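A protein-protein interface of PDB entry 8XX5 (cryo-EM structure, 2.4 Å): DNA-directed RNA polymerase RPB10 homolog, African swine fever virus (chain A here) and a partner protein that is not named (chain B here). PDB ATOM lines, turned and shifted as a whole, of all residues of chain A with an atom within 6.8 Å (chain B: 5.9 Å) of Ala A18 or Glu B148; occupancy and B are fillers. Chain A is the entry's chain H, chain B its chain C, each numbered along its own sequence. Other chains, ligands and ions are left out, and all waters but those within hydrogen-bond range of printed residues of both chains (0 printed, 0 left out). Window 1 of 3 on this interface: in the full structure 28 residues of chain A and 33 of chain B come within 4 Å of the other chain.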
ATOM      1  N   LEU A   2      19.946 -27.162 -13.489  1.00  0.00           N
ATOM      2  CA  LEU A   2      21.163 -26.493 -13.063  1.00  0.00           C
ATOM      3  C   LEU A   2      20.869 -25.008 -12.927  1.00  0.00           C
ATOM      4  O   LEU A   2      19.832 -24.518 -13.382  1.00  0.00           O
ATOM      5  CB  LEU A   2      22.313 -26.714 -14.055  1.00  0.00           C
ATOM      6  CG  LEU A   2      22.819 -28.138 -14.275  1.00  0.00           C
ATOM      7  CD1 LEU A   2      23.500 -28.259 -15.626  1.00  0.00           C
ATOM      8  CD2 LEU A   2      23.769 -28.538 -13.166  1.00  0.00           C
ATOM      9  N   ILE A   3      21.786 -24.290 -12.288  1.00  0.00           N
ATOM     10  CA  ILE A   3      21.690 -22.828 -12.335  1.00  0.00           C
ATOM     11  C   ILE A   3      21.808 -22.387 -13.787  1.00  0.00           C
ATOM     12  O   ILE A   3      22.727 -22.841 -14.496  1.00  0.00           O
ATOM     13  CB  ILE A   3      22.782 -22.181 -11.467  1.00  0.00           C
ATOM     14  CG1 ILE A   3      22.452 -22.339  -9.984  1.00  0.00           C
ATOM     15  CG2 ILE A   3      22.936 -20.708 -11.806  1.00  0.00           C
ATOM     16  CD1 ILE A   3      23.539 -21.842  -9.062  1.00  0.00           C
ATOM     17  N   PRO A   4      20.913 -21.536 -14.288  1.00  0.00           N
ATOM     18  CA  PRO A   4      20.919 -21.222 -15.720  1.00  0.00           C
ATOM     19  C   PRO A   4      22.224 -20.574 -16.154  1.00  0.00           C
ATOM     20  O   PRO A   4      22.909 -19.914 -15.371  1.00  0.00           O
ATOM     21  CB  PRO A   4      19.735 -20.261 -15.879  1.00  0.00           C
ATOM     22  CG  PRO A   4      19.469 -19.740 -14.508  1.00  0.00           C
ATOM     23  CD  PRO A   4      19.823 -20.849 -13.577  1.00  0.00           C
ATOM     24  N   VAL A   5      22.573 -20.800 -17.422  1.00  0.00           N
ATOM     25  CA  VAL A   5      23.800 -20.238 -17.979  1.00  0.00           C
ATOM     26  C   VAL A   5      23.776 -18.719 -17.890  1.00  0.00           C
ATOM     27  O   VAL A   5      24.777 -18.085 -17.537  1.00  0.00           O
ATOM     28  CB  VAL A   5      23.991 -20.721 -19.429  1.00  0.00           C
ATOM     29  CG1 VAL A   5      25.090 -19.936 -20.113  1.00  0.00           C
ATOM     30  CG2 VAL A   5      24.304 -22.204 -19.452  1.00  0.00           C
ATOM     31  N   PRO A  13      25.435 -13.351 -17.716  1.00  0.00           N
ATOM     32  CA  PRO A  13      25.989 -14.704 -17.572  1.00  0.00           C
ATOM     33  C   PRO A  13      26.234 -15.110 -16.128  1.00  0.00           C
ATOM     34  O   PRO A  13      27.382 -15.155 -15.678  1.00  0.00           O
ATOM     35  CB  PRO A  13      27.304 -14.623 -18.352  1.00  0.00           C
ATOM     36  CG  PRO A  13      27.682 -13.188 -18.291  1.00  0.00           C
ATOM     37  CD  PRO A  13      26.396 -12.423 -18.334  1.00  0.00           C
ATOM     38  N   ILE A  14      25.162 -15.414 -15.391  1.00  0.00           N
ATOM     39  CA  ILE A  14      25.321 -15.869 -14.016  1.00  0.00           C
ATOM     40  C   ILE A  14      25.902 -17.274 -13.951  1.00  0.00           C
ATOM     41  O   ILE A  14      26.431 -17.673 -12.908  1.00  0.00           O
ATOM     42  CB  ILE A  14      23.979 -15.804 -13.265  1.00  0.00           C
ATOM     43  CG1 ILE A  14      22.900 -16.578 -14.024  1.00  0.00           C
ATOM     44  CG2 ILE A  14      23.559 -14.361 -13.056  1.00  0.00           C
ATOM     45  CD1 ILE A  14      21.774 -17.067 -13.148  1.00  0.00           C
ATOM     46  N   GLY A  15      25.828 -18.035 -15.041  1.00  0.00           N
ATOM     47  CA  GLY A  15      26.361 -19.385 -15.054  1.00  0.00           C
ATOM     48  C   GLY A  15      27.870 -19.461 -15.091  1.00  0.00           C
ATOM     49  O   GLY A  15      28.421 -20.552 -14.910  1.00  0.00           O
ATOM     50  N   THR A  16      28.549 -18.336 -15.329  1.00  0.00           N
ATOM     51  CA  THR A  16      30.005 -18.321 -15.262  1.00  0.00           C
ATOM     52  C   THR A  16      30.499 -18.623 -13.856  1.00  0.00           C
ATOM     53  O   THR A  16      31.557 -19.237 -13.685  1.00  0.00           O
ATOM     54  CB  THR A  16      30.537 -16.963 -15.718  1.00  0.00           C
ATOM     55  OG1 THR A  16      29.636 -16.391 -16.672  1.00  0.00           O
ATOM     56  CG2 THR A  16      31.904 -17.117 -16.349  1.00  0.00           C
ATOM     57  N   TYR A  17      29.751 -18.199 -12.841  1.00  0.00           N
ATOM     58  CA  TYR A  17      30.128 -18.380 -11.448  1.00  0.00           C
ATOM     59  C   TYR A  17      29.206 -19.343 -10.715  1.00  0.00           C
ATOM     60  O   TYR A  17      29.247 -19.406  -9.484  1.00  0.00           O
ATOM     61  CB  TYR A  17      30.144 -17.026 -10.735  1.00  0.00           C
ATOM     62  CG  TYR A  17      30.501 -15.870 -11.639  1.00  0.00           C
ATOM     63  CD1 TYR A  17      31.827 -15.555 -11.905  1.00  0.00           C
ATOM     64  CD2 TYR A  17      29.513 -15.097 -12.232  1.00  0.00           C
ATOM     65  CE1 TYR A  17      32.158 -14.502 -12.732  1.00  0.00           C
ATOM     66  CE2 TYR A  17      29.834 -14.043 -13.061  1.00  0.00           C
ATOM     67  CZ  TYR A  17      31.157 -13.749 -13.307  1.00  0.00           C
ATOM     68  OH  TYR A  17      31.479 -12.697 -14.132  1.00  0.00           O
ATOM     69  N   ALA A  18      28.378 -20.096 -11.444  1.00  0.00           N
ATOM     70  CA  ALA A  18      27.378 -20.945 -10.805  1.00  0.00           C
ATOM     71  C   ALA A  18      28.026 -22.038  -9.963  1.00  0.00           C
ATOM     72  O   ALA A  18      27.619 -22.280  -8.821  1.00  0.00           O
ATOM     73  CB  ALA A  18      26.462 -21.555 -11.865  1.00  0.00           C
ATOM     74  N   ALA A  19      29.038 -22.712 -10.509  1.00  0.00           N
ATOM     75  CA  ALA A  19      29.704 -23.776  -9.764  1.00  0.00           C
ATOM     76  C   ALA A  19      30.462 -23.215  -8.567  1.00  0.00           C
ATOM     77  O   ALA A  19      30.385 -23.756  -7.455  1.00  0.00           O
ATOM     78  CB  ALA A  19      30.644 -24.549 -10.688  1.00  0.00           C
ATOM     79  N   ILE A  20      31.203 -22.125  -8.782  1.00  0.00           N
ATOM     80  CA  ILE A  20      31.928 -21.484  -7.692  1.00  0.00           C
ATOM     81  C   ILE A  20      30.957 -20.992  -6.632  1.00  0.00           C
ATOM     82  O   ILE A  20      31.201 -21.144  -5.429  1.00  0.00           O
ATOM     83  CB  ILE A  20      32.809 -20.342  -8.231  1.00  0.00           C
ATOM     84  CG1 ILE A  20      33.845 -20.884  -9.214  1.00  0.00           C
ATOM     85  CG2 ILE A  20      33.497 -19.612  -7.090  1.00  0.00           C
ATOM     86  CD1 ILE A  20      34.457 -19.827 -10.100  1.00  0.00           C
ATOM     87  N   PHE A  21      29.840 -20.394  -7.056  1.00  0.00           N
ATOM     88  CA  PHE A  21      28.845 -19.939  -6.092  1.00  0.00           C
ATOM     89  C   PHE A  21      28.286 -21.097  -5.284  1.00  0.00           C
ATOM     90  O   PHE A  21      28.128 -20.986  -4.068  1.00  0.00           O
ATOM     91  CB  PHE A  21      27.697 -19.214  -6.785  1.00  0.00           C
ATOM     92  CG  PHE A  21      26.564 -18.889  -5.861  1.00  0.00           C
ATOM     93  CD1 PHE A  21      26.713 -17.925  -4.880  1.00  0.00           C
ATOM     94  CD2 PHE A  21      25.363 -19.566  -5.949  1.00  0.00           C
ATOM     95  CE1 PHE A  21      25.681 -17.632  -4.019  1.00  0.00           C
ATOM     96  CE2 PHE A  21      24.326 -19.274  -5.090  1.00  0.00           C
ATOM     97  CZ  PHE A  21      24.487 -18.307  -4.125  1.00  0.00           C
ATOM     98  N   ASP A  22      27.957 -22.206  -5.946  1.00  0.00           N
ATOM     99  CA  ASP A  22      27.383 -23.346  -5.240  1.00  0.00           C
ATOM    100  C   ASP A  22      28.357 -23.889  -4.203  1.00  0.00           C
ATOM    101  O   ASP A  22      27.989 -24.126  -3.044  1.00  0.00           O
ATOM    102  CB  ASP A  22      26.995 -24.429  -6.247  1.00  0.00           C
ATOM    103  CG  ASP A  22      26.132 -25.509  -5.636  1.00  0.00           C
ATOM    104  OD1 ASP A  22      26.696 -26.489  -5.106  1.00  0.00           O
ATOM    105  OD2 ASP A  22      24.892 -25.378  -5.687  1.00  0.00           O
ATOM    106  N   LYS A  23      29.621 -24.061  -4.597  1.00  0.00           N
ATOM    107  CA  LYS A  23      30.617 -24.576  -3.662  1.00  0.00           C
ATOM    108  C   LYS A  23      30.834 -23.616  -2.498  1.00  0.00           C
ATOM    109  O   LYS A  23      30.847 -24.033  -1.332  1.00  0.00           O
ATOM    110  CB  LYS A  23      31.931 -24.838  -4.390  1.00  0.00           C
ATOM    111  CG  LYS A  23      32.167 -26.292  -4.708  1.00  0.00           C
ATOM    112  CD  LYS A  23      33.637 -26.606  -4.609  1.00  0.00           C
ATOM    113  CE  LYS A  23      34.090 -26.461  -3.171  1.00  0.00           C
ATOM    114  NZ  LYS A  23      33.303 -27.327  -2.251  1.00  0.00           N
ATOM    115  N   ARG A  25      28.844 -21.333  -1.358  1.00  0.00           N
ATOM    116  CA  ARG A  25      27.653 -21.298  -0.521  1.00  0.00           C
ATOM    117  C   ARG A  25      27.598 -22.504   0.400  1.00  0.00           C
ATOM    118  O   ARG A  25      27.221 -22.376   1.568  1.00  0.00           O
ATOM    119  CB  ARG A  25      26.396 -21.225  -1.389  1.00  0.00           C
ATOM    120  CG  ARG A  25      25.115 -21.477  -0.615  1.00  0.00           C
ATOM    121  CD  ARG A  25      23.881 -21.251  -1.460  1.00  0.00           C
ATOM    122  NE  ARG A  25      23.849 -22.115  -2.633  1.00  0.00           N
ATOM    123  CZ  ARG A  25      22.907 -22.069  -3.564  1.00  0.00           C
ATOM    124  NH1 ARG A  25      21.901 -21.216  -3.485  1.00  0.00           N
ATOM    125  NH2 ARG A  25      22.977 -22.900  -4.600  1.00  0.00           N
ATOM    126  N   LEU A  58      31.825 -12.587  -6.105  1.00  0.00           N
ATOM    127  CA  LEU A  58      31.842 -13.277  -7.388  1.00  0.00           C
ATOM    128  C   LEU A  58      31.901 -12.329  -8.577  1.00  0.00           C
ATOM    129  O   LEU A  58      32.182 -12.780  -9.691  1.00  0.00           O
ATOM    130  CB  LEU A  58      30.613 -14.169  -7.518  1.00  0.00           C
ATOM    131  CG  LEU A  58      30.753 -15.571  -6.942  1.00  0.00           C
ATOM    132  CD1 LEU A  58      29.460 -16.301  -7.145  1.00  0.00           C
ATOM    133  CD2 LEU A  58      31.902 -16.309  -7.602  1.00  0.00           C
ATOM    134  N   ILE A  60      29.220 -10.645  -9.609  1.00  0.00           N
ATOM    135  CA  ILE A  60      27.846 -10.456 -10.083  1.00  0.00           C
ATOM    136  C   ILE A  60      27.322  -9.121  -9.563  1.00  0.00           C
ATOM    137  O   ILE A  60      27.507  -8.808  -8.374  1.00  0.00           O
ATOM    138  CB  ILE A  60      26.965 -11.619  -9.624  1.00  0.00           C
ATOM    139  CG1 ILE A  60      27.320 -12.885 -10.403  1.00  0.00           C
ATOM    140  CG2 ILE A  60      25.491 -11.292  -9.792  1.00  0.00           C
ATOM    141  CD1 ILE A  60      27.436 -14.116  -9.542  1.00  0.00           C
ATOM    142  N   LEU A  70      20.491 -16.872  -9.150  1.00  0.00           N
ATOM    143  CA  LEU A  70      21.683 -17.560  -8.673  1.00  0.00           C
ATOM    144  C   LEU A  70      21.415 -18.306  -7.373  1.00  0.00           C
ATOM    145  O   LEU A  70      21.832 -19.457  -7.216  1.00  0.00           O
ATOM    146  CB  LEU A  70      22.823 -16.561  -8.493  1.00  0.00           C
ATOM    147  CG  LEU A  70      24.196 -17.161  -8.213  1.00  0.00           C
ATOM    148  CD1 LEU A  70      24.803 -17.729  -9.484  1.00  0.00           C
ATOM    149  CD2 LEU A  70      25.110 -16.122  -7.594  1.00  0.00           C
ATOM    150  N   ASP A  75      19.397 -27.479  -8.028  1.00  0.00           N
ATOM    151  CA  ASP A  75      20.320 -28.356  -8.732  1.00  0.00           C
ATOM    152  C   ASP A  75      19.764 -29.772  -8.721  1.00  0.00           C
ATOM    153  O   ASP A  75      19.460 -30.315  -7.654  1.00  0.00           O
ATOM    154  CB  ASP A  75      21.705 -28.322  -8.088  1.00  0.00           C
ATOM    155  CG  ASP A  75      22.794 -28.797  -9.025  1.00  0.00           C
ATOM    156  OD1 ASP A  75      22.467 -29.252 -10.140  1.00  0.00           O
ATOM    157  OD2 ASP A  75      23.980 -28.717  -8.645  1.00  0.00           O
ATOM    158  N   ARG A  77      21.203 -32.661  -9.455  1.00  0.00           N
ATOM    159  CA  ARG A  77      22.053 -33.701  -8.888  1.00  0.00           C
ATOM    160  C   ARG A  77      22.020 -33.717  -7.366  1.00  0.00           C
ATOM    161  O   ARG A  77      22.408 -34.722  -6.764  1.00  0.00           O
ATOM    162  CB  ARG A  77      23.498 -33.546  -9.365  1.00  0.00           C
ATOM    163  CG  ARG A  77      23.928 -32.135  -9.684  1.00  0.00           C
ATOM    164  CD  ARG A  77      25.007 -32.137 -10.751  1.00  0.00           C
ATOM    165  NE  ARG A  77      25.330 -30.791 -11.207  1.00  0.00           N
ATOM    166  CZ  ARG A  77      26.133 -29.957 -10.561  1.00  0.00           C
ATOM    167  NH1 ARG A  77      26.722 -30.304  -9.429  1.00  0.00           N
ATOM    168  NH2 ARG A  77      26.352 -28.746 -11.063  1.00  0.00           N
ATOM    169  N   ARG B  96      21.520 -24.761 -22.878  1.00  0.00           N
ATOM    170  CA  ARG B  96      22.704 -24.331 -22.136  1.00  0.00           C
ATOM    171  C   ARG B  96      23.781 -23.792 -23.070  1.00  0.00           C
ATOM    172  O   ARG B  96      24.404 -22.763 -22.786  1.00  0.00           O
ATOM    173  CB  ARG B  96      23.274 -25.475 -21.293  1.00  0.00           C
ATOM    174  CG  ARG B  96      22.256 -26.301 -20.542  1.00  0.00           C
ATOM    175  CD  ARG B  96      21.968 -25.757 -19.161  1.00  0.00           C
ATOM    176  NE  ARG B  96      23.168 -25.548 -18.365  1.00  0.00           N
ATOM    177  CZ  ARG B  96      23.198 -24.859 -17.234  1.00  0.00           C
ATOM    178  NH1 ARG B  96      22.105 -24.304 -16.736  1.00  0.00           N
ATOM    179  NH2 ARG B  96      24.349 -24.723 -16.585  1.00  0.00           N
ATOM    180  N   THR B 124      30.148 -33.669 -13.710  1.00  0.00           N
ATOM    181  CA  THR B 124      29.678 -32.426 -14.301  1.00  0.00           C
ATOM    182  C   THR B 124      30.478 -32.110 -15.557  1.00  0.00           C
ATOM    183  O   THR B 124      31.703 -32.251 -15.581  1.00  0.00           O
ATOM    184  CB  THR B 124      29.797 -31.274 -13.303  1.00  0.00           C
ATOM    185  OG1 THR B 124      29.232 -31.668 -12.046  1.00  0.00           O
ATOM    186  CG2 THR B 124      29.066 -30.046 -13.813  1.00  0.00           C
ATOM    187  N   ILE B 125      29.774 -31.687 -16.602  1.00  0.00           N
ATOM    188  CA  ILE B 125      30.393 -31.286 -17.859  1.00  0.00           C
ATOM    189  C   ILE B 125      30.543 -29.774 -17.842  1.00  0.00           C
ATOM    190  O   ILE B 125      29.565 -29.045 -17.639  1.00  0.00           O
ATOM    191  CB  ILE B 125      29.566 -31.742 -19.069  1.00  0.00           C
ATOM    192  CG1 ILE B 125      29.137 -33.200 -18.910  1.00  0.00           C
ATOM    193  CG2 ILE B 125      30.358 -31.554 -20.353  1.00  0.00           C
ATOM    194  CD1 ILE B 125      27.774 -33.494 -19.490  1.00  0.00           C
ATOM    195  N   TYR B 126      31.763 -29.300 -18.051  1.00  0.00           N
ATOM    196  CA  TYR B 126      32.052 -27.877 -18.073  1.00  0.00           C
ATOM    197  C   TYR B 126      32.372 -27.427 -19.492  1.00  0.00           C
ATOM    198  O   TYR B 126      32.682 -28.236 -20.368  1.00  0.00           O
ATOM    199  CB  TYR B 126      33.208 -27.540 -17.127  1.00  0.00           C
ATOM    200  CG  TYR B 126      32.842 -27.700 -15.672  1.00  0.00           C
ATOM    201  CD1 TYR B 126      31.971 -26.813 -15.056  1.00  0.00           C
ATOM    202  CD2 TYR B 126      33.356 -28.744 -14.917  1.00  0.00           C
ATOM    203  CE1 TYR B 126      31.627 -26.956 -13.729  1.00  0.00           C
ATOM    204  CE2 TYR B 126      33.018 -28.895 -13.587  1.00  0.00           C
ATOM    205  CZ  TYR B 126      32.153 -27.999 -13.000  1.00  0.00           C
ATOM    206  OH  TYR B 126      31.811 -28.143 -11.675  1.00  0.00           O
ATOM    207  N   SER B 127      32.275 -26.114 -19.712  1.00  0.00           N
ATOM    208  CA  SER B 127      32.602 -25.563 -21.021  1.00  0.00           C
ATOM    209  C   SER B 127      34.073 -25.748 -21.364  1.00  0.00           C
ATOM    210  O   SER B 127      34.442 -25.641 -22.538  1.00  0.00           O
ATOM    211  CB  SER B 127      32.226 -24.082 -21.082  1.00  0.00           C
ATOM    212  OG  SER B 127      32.448 -23.447 -19.838  1.00  0.00           O
ATOM    213  N   THR B 146      34.086 -22.082 -17.219  1.00  0.00           N
ATOM    214  CA  THR B 146      33.479 -22.422 -15.940  1.00  0.00           C
ATOM    215  C   THR B 146      31.989 -22.727 -16.033  1.00  0.00           C
ATOM    216  O   THR B 146      31.367 -23.000 -15.003  1.00  0.00           O
ATOM    217  CB  THR B 146      33.706 -21.287 -14.937  1.00  0.00           C
ATOM    218  OG1 THR B 146      33.213 -20.059 -15.482  1.00  0.00           O
ATOM    219  CG2 THR B 146      35.184 -21.141 -14.628  1.00  0.00           C
ATOM    220  N   PHE B 147      31.402 -22.686 -17.224  1.00  0.00           N
ATOM    221  CA  PHE B 147      29.981 -22.972 -17.361  1.00  0.00           C
ATOM    222  C   PHE B 147      29.715 -24.461 -17.182  1.00  0.00           C
ATOM    223  O   PHE B 147      30.435 -25.302 -17.720  1.00  0.00           O
ATOM    224  CB  PHE B 147      29.472 -22.524 -18.729  1.00  0.00           C
ATOM    225  CG  PHE B 147      29.426 -21.038 -18.899  1.00  0.00           C
ATOM    226  CD1 PHE B 147      30.522 -20.351 -19.389  1.00  0.00           C
ATOM    227  CD2 PHE B 147      28.286 -20.326 -18.576  1.00  0.00           C
ATOM    228  CE1 PHE B 147      30.484 -18.987 -19.548  1.00  0.00           C
ATOM    229  CE2 PHE B 147      28.241 -18.959 -18.735  1.00  0.00           C
ATOM    230  CZ  PHE B 147      29.343 -18.289 -19.221  1.00  0.00           C
ATOM    231  N   GLU B 148      28.665 -24.785 -16.431  1.00  0.00           N
ATOM    232  CA  GLU B 148      28.213 -26.167 -16.283  1.00  0.00           C
ATOM    233  C   GLU B 148      27.247 -26.468 -17.420  1.00  0.00           C
ATOM    234  O   GLU B 148      26.097 -26.028 -17.405  1.00  0.00           O
ATOM    235  CB  GLU B 148      27.551 -26.389 -14.929  1.00  0.00           C
ATOM    236  CG  GLU B 148      28.262 -25.750 -13.755  1.00  0.00           C
ATOM    237  CD  GLU B 148      27.470 -25.874 -12.469  1.00  0.00           C
ATOM    238  OE1 GLU B 148      26.394 -25.248 -12.369  1.00  0.00           O
ATOM    239  OE2 GLU B 148      27.920 -26.602 -11.561  1.00  0.00           O
ATOM    240  N   ILE B 149      27.717 -27.214 -18.420  1.00  0.00           N
ATOM    241  CA  ILE B 149      26.836 -27.610 -19.512  1.00  0.00           C
ATOM    242  C   ILE B 149      25.820 -28.636 -19.030  1.00  0.00           C
ATOM    243  O   ILE B 149      24.624 -28.534 -19.326  1.00  0.00           O
ATOM    244  CB  ILE B 149      27.662 -28.137 -20.697  1.00  0.00           C
ATOM    245  CG1 ILE B 149      28.545 -27.024 -21.263  1.00  0.00           C
ATOM    246  CG2 ILE B 149      26.751 -28.696 -21.775  1.00  0.00           C
ATOM    247  CD1 ILE B 149      29.663 -27.524 -22.140  1.00  0.00           C
ATOM    248  N   GLY B 150      26.272 -29.627 -18.275  1.00  0.00           N
ATOM    249  CA  GLY B 150      25.379 -30.656 -17.778  1.00  0.00           C
ATOM    250  C   GLY B 150      26.137 -31.616 -16.894  1.00  0.00           C
ATOM    251  O   GLY B 150      27.324 -31.432 -16.607  1.00  0.00           O
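N of Gly A15 lies within hydrogen-bond range of O of Val A5. The guanidinium group (NE) of Arg B96 sits at hydrogen-bond distance from the backbone carbonyl oxygen (O) of Glu B148, 3.1 Å away. The backbone NH of Gly A15 is in hydrogen-bond range of the backbone carbonyl oxygen of Pro A4 (3.5 Å). O of Ile B125 is in hydrogen-bond range of N of Ile B149. The guanidinium group (NE) of Arg B96 is in hydrogen-bond range of the backbone carbonyl oxygen (O) of Ile B149 (3.5 Å). O of Val A5 is in hydrogen-bond range of N of Ile A14 (3.4 Å).
OE2 of Glu B148 is in salt-bridge range of NH2 of Arg A77, at 2.7 Å. The backbone carbonyl oxygen (O) of Ile A3 is in hydrogen-bond range of the guanidinium group (NH1) of Arg B96. OG1 of Thr B146 lies within hydrogen-bond range of O of Thr A16, 2.6 Å away.
Of chain B, only Glu B148 comes within 4 Å of Ala A18. Glu B148 touches four residues of chain A. Printed residues of chain B within 4 Å of Arg A77: Thr B124 and Glu B148. Of the printed residues of chain A, Thr B146 touches Gly A15 (3.8 Å) and Thr A16 (2.6 Å). The nearest residue of chain B that does not touch Ala A18 is Thr B146 (5.5 Å). The nearest printed residue of chain B that does not touch Val A5 is Glu B148 (4.7 Å).
Of the 21 printed residues of chain A, 9 touch a printed residue of chain B. Printed residues of chain B that touch a printed residue of chain A: Arg B96, Thr B124, Tyr B126, Thr B146, Phe B147, Glu B148, Ile B149 and Gly B150. Hydrophobic or aromatic side chains of chain B that line the printed part of chain A: Tyr B126 and Phe B147. Among the printed residues, 17 pairs touch across the chains. Among the printed residues, Asp or Glu carboxylates within 4 Å of a Lys or Arg side-chain nitrogen of the other chain: Arg A77 with Glu B148.
Leu A2 touches Arg B96 (CB to NH1, 3.6 Å). Leu A2 touches Glu B148 (CD1 to O, 3.9 Å). Leu A2 touches Ile B149 (CD1 to O, 3.9 Å). Gly B150 touches Leu A2. Phe B147 touches Val A5. Gly A15 touches Thr B146 (O to O, 3.8 Å). Thr A16 touches Phe B147. Glu B148 touches Ala A18. Ala A19 touches Glu B148. CZ of Arg A77 touches OG1 of Thr B124 (3.8 Å).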
